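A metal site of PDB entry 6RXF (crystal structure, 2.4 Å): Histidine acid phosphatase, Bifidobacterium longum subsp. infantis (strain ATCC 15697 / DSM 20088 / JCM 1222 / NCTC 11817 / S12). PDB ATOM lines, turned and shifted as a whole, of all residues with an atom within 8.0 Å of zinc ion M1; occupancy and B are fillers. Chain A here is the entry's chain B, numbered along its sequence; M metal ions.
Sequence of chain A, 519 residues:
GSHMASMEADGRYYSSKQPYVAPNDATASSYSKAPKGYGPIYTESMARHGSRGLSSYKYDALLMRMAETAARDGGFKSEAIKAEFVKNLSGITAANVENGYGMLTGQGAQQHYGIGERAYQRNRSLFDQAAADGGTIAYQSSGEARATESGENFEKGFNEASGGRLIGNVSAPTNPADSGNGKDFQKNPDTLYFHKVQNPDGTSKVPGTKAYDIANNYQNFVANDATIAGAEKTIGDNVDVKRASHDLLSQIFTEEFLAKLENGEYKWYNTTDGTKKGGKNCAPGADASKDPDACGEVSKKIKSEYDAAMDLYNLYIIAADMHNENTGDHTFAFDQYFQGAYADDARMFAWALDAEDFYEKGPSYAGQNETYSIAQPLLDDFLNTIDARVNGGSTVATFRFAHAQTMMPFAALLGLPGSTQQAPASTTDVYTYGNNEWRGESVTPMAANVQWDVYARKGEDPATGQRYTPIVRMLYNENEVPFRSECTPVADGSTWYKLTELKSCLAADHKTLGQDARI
Zinc ion M1 is bound by OE2 of Glu 356, OE2 of Glu 360 and OE2 of Glu 232. Zinc ion M1 has three donor atoms within binding distance. Slightly farther from zinc ion M1 lies the side-chain carboxylate (OE1) of Glu 232 (2.8 Å).
OE1 of Glu 360 lies within salt-bridge range of NZ of Lys 361 (2.8 Å).
Of the 12 residues printed, 3 come within 4 Å of zinc ion M1.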
ATOM      1  N   VAL A 222       1.623  31.240  11.575  1.00  0.00           N
ATOM      2  CA  VAL A 222       0.805  30.666  12.642  1.00  0.00           C
ATOM      3  C   VAL A 222       0.289  31.750  13.577  1.00  0.00           C
ATOM      4  O   VAL A 222      -0.872  31.712  14.009  1.00  0.00           O
ATOM      5  CB  VAL A 222       1.611  29.583  13.397  1.00  0.00           C
ATOM      6  CG1 VAL A 222       1.068  29.380  14.797  1.00  0.00           C
ATOM      7  CG2 VAL A 222       1.550  28.278  12.625  1.00  0.00           C
ATOM      8  N   ALA A 223       1.112  32.746  13.895  1.00  0.00           N
ATOM      9  CA  ALA A 223       0.678  33.804  14.804  1.00  0.00           C
ATOM     10  C   ALA A 223      -0.374  34.711  14.187  1.00  0.00           C
ATOM     11  O   ALA A 223      -1.127  35.357  14.934  1.00  0.00           O
ATOM     12  CB  ALA A 223       1.879  34.628  15.264  1.00  0.00           C
ATOM     13  N   ILE A 228      -6.992  29.919  11.111  1.00  0.00           N
ATOM     14  CA  ILE A 228      -6.616  29.203  12.330  1.00  0.00           C
ATOM     15  C   ILE A 228      -7.179  29.917  13.550  1.00  0.00           C
ATOM     16  O   ILE A 228      -7.738  29.280  14.457  1.00  0.00           O
ATOM     17  CB  ILE A 228      -5.083  29.057  12.412  1.00  0.00           C
ATOM     18  CG1 ILE A 228      -4.570  28.116  11.326  1.00  0.00           C
ATOM     19  CG2 ILE A 228      -4.678  28.556  13.796  1.00  0.00           C
ATOM     20  CD1 ILE A 228      -3.065  28.133  11.152  1.00  0.00           C
ATOM     21  N   ALA A 229      -7.049  31.240  13.603  1.00  0.00           N
ATOM     22  CA  ALA A 229      -7.525  32.003  14.743  1.00  0.00           C
ATOM     23  C   ALA A 229      -9.032  31.842  14.932  1.00  0.00           C
ATOM     24  O   ALA A 229      -9.510  31.705  16.061  1.00  0.00           O
ATOM     25  CB  ALA A 229      -7.172  33.486  14.572  1.00  0.00           C
ATOM     26  N   GLU A 232      -9.857  28.138  16.085  1.00  0.00           N
ATOM     27  CA  GLU A 232      -9.519  27.910  17.483  1.00  0.00           C
ATOM     28  C   GLU A 232     -10.440  28.676  18.425  1.00  0.00           C
ATOM     29  O   GLU A 232     -10.728  28.221  19.535  1.00  0.00           O
ATOM     30  CB  GLU A 232      -8.062  28.300  17.742  1.00  0.00           C
ATOM     31  CG  GLU A 232      -7.050  27.236  17.275  1.00  0.00           C
ATOM     32  CD  GLU A 232      -5.677  27.398  17.879  1.00  0.00           C
ATOM     33  OE1 GLU A 232      -5.291  26.554  18.710  1.00  0.00           O
ATOM     34  OE2 GLU A 232      -4.976  28.368  17.508  1.00  0.00           O
ATOM     35  N   LYS A 233     -10.903  29.855  17.998  1.00  0.00           N
ATOM     36  CA  LYS A 233     -11.924  30.553  18.767  1.00  0.00           C
ATOM     37  C   LYS A 233     -13.214  29.741  18.819  1.00  0.00           C
ATOM     38  O   LYS A 233     -13.853  29.647  19.873  1.00  0.00           O
ATOM     39  CB  LYS A 233     -12.175  31.933  18.150  1.00  0.00           C
ATOM     40  CG  LYS A 233     -12.949  32.883  19.039  1.00  0.00           C
ATOM     41  CD  LYS A 233     -14.291  33.279  18.418  1.00  0.00           C
ATOM     42  CE  LYS A 233     -14.949  34.416  19.196  1.00  0.00           C
ATOM     43  NZ  LYS A 233     -15.131  34.078  20.646  1.00  0.00           N
ATOM     44  N   ALA A 355      -6.967  19.464  18.545  1.00  0.00           N
ATOM     45  CA  ALA A 355      -7.354  20.495  17.606  1.00  0.00           C
ATOM     46  C   ALA A 355      -6.260  21.541  17.418  1.00  0.00           C
ATOM     47  O   ALA A 355      -5.881  21.868  16.286  1.00  0.00           O
ATOM     48  CB  ALA A 355      -8.671  21.146  18.043  1.00  0.00           C
ATOM     49  N   GLU A 356      -5.725  22.072  18.531  1.00  0.00           N
ATOM     50  CA  GLU A 356      -4.658  23.072  18.449  1.00  0.00           C
ATOM     51  C   GLU A 356      -3.439  22.533  17.708  1.00  0.00           C
ATOM     52  O   GLU A 356      -2.844  23.210  16.859  1.00  0.00           O
ATOM     53  CB  GLU A 356      -4.259  23.539  19.851  1.00  0.00           C
ATOM     54  CG  GLU A 356      -2.972  24.373  19.858  1.00  0.00           C
ATOM     55  OE1 GLU A 356      -3.736  25.663  21.694  1.00  0.00           O
ATOM     56  OE2 GLU A 356      -2.616  26.697  20.130  1.00  0.00           O
ATOM     57  N   ASP A 357      -3.042  21.315  18.080  1.00  0.00           N
ATOM     58  CA  ASP A 357      -1.942  20.646  17.392  1.00  0.00           C
ATOM     59  C   ASP A 357      -2.263  20.428  15.909  1.00  0.00           C
ATOM     60  O   ASP A 357      -1.408  20.672  15.046  1.00  0.00           O
ATOM     61  CB  ASP A 357      -1.638  19.318  18.079  1.00  0.00           C
ATOM     62  CG  ASP A 357      -0.603  19.458  19.182  1.00  0.00           C
ATOM     63  OD1 ASP A 357       0.164  20.430  19.147  1.00  0.00           O
ATOM     64  OD2 ASP A 357      -0.533  18.567  20.069  1.00  0.00           O
ATOM     65  N   TYR A 359      -4.268  22.066  13.841  1.00  0.00           N
ATOM     66  CA  TYR A 359      -4.299  23.282  13.044  1.00  0.00           C
ATOM     67  C   TYR A 359      -2.941  23.968  12.953  1.00  0.00           C
ATOM     68  O   TYR A 359      -2.723  24.732  12.002  1.00  0.00           O
ATOM     69  CB  TYR A 359      -5.302  24.277  13.617  1.00  0.00           C
ATOM     70  CG  TYR A 359      -6.734  24.020  13.203  1.00  0.00           C
ATOM     71  CD1 TYR A 359      -7.141  24.192  11.880  1.00  0.00           C
ATOM     72  CD2 TYR A 359      -7.673  23.588  14.122  1.00  0.00           C
ATOM     73  CE1 TYR A 359      -8.442  23.955  11.498  1.00  0.00           C
ATOM     74  CE2 TYR A 359      -8.972  23.347  13.759  1.00  0.00           C
ATOM     75  CZ  TYR A 359      -9.352  23.529  12.446  1.00  0.00           C
ATOM     76  OH  TYR A 359     -10.659  23.288  12.095  1.00  0.00           O
ATOM     77  N   GLU A 360      -2.025  23.720  13.888  1.00  0.00           N
ATOM     78  CA  GLU A 360      -0.768  24.452  13.913  1.00  0.00           C
ATOM     79  C   GLU A 360       0.417  23.651  13.390  1.00  0.00           C
ATOM     80  O   GLU A 360       1.339  24.242  12.825  1.00  0.00           O
ATOM     81  CB  GLU A 360      -0.468  24.929  15.340  1.00  0.00           C
ATOM     82  CG  GLU A 360      -1.460  25.966  15.849  1.00  0.00           C
ATOM     83  CD  GLU A 360      -1.072  26.523  17.204  1.00  0.00           C
ATOM     84  OE1 GLU A 360      -0.171  25.950  17.850  1.00  0.00           O
ATOM     85  OE2 GLU A 360      -1.671  27.542  17.613  1.00  0.00           O
ATOM     86  N   LYS A 361       0.408  22.332  13.563  1.00  0.00           N
ATOM     87  CA  LYS A 361       1.531  21.512  13.136  1.00  0.00           C
ATOM     88  C   LYS A 361       1.140  20.359  12.232  1.00  0.00           C
ATOM     89  O   LYS A 361       2.036  19.706  11.675  1.00  0.00           O
ATOM     90  CB  LYS A 361       2.292  20.957  14.352  1.00  0.00           C
ATOM     91  CG  LYS A 361       2.795  22.021  15.325  1.00  0.00           C
ATOM     92  CD  LYS A 361       2.067  21.944  16.663  1.00  0.00           C
ATOM     93  CE  LYS A 361       2.561  23.011  17.637  1.00  0.00           C
ATOM     94  NZ  LYS A 361       2.090  24.384  17.282  1.00  0.00           N
HETATM   95 ZN    ZN M   1      -3.151  28.386  19.125  1.00  0.00          ZN
HETATM   96 ZN    ZN M   2      -3.615  31.121  17.528  1.00  0.00          ZN
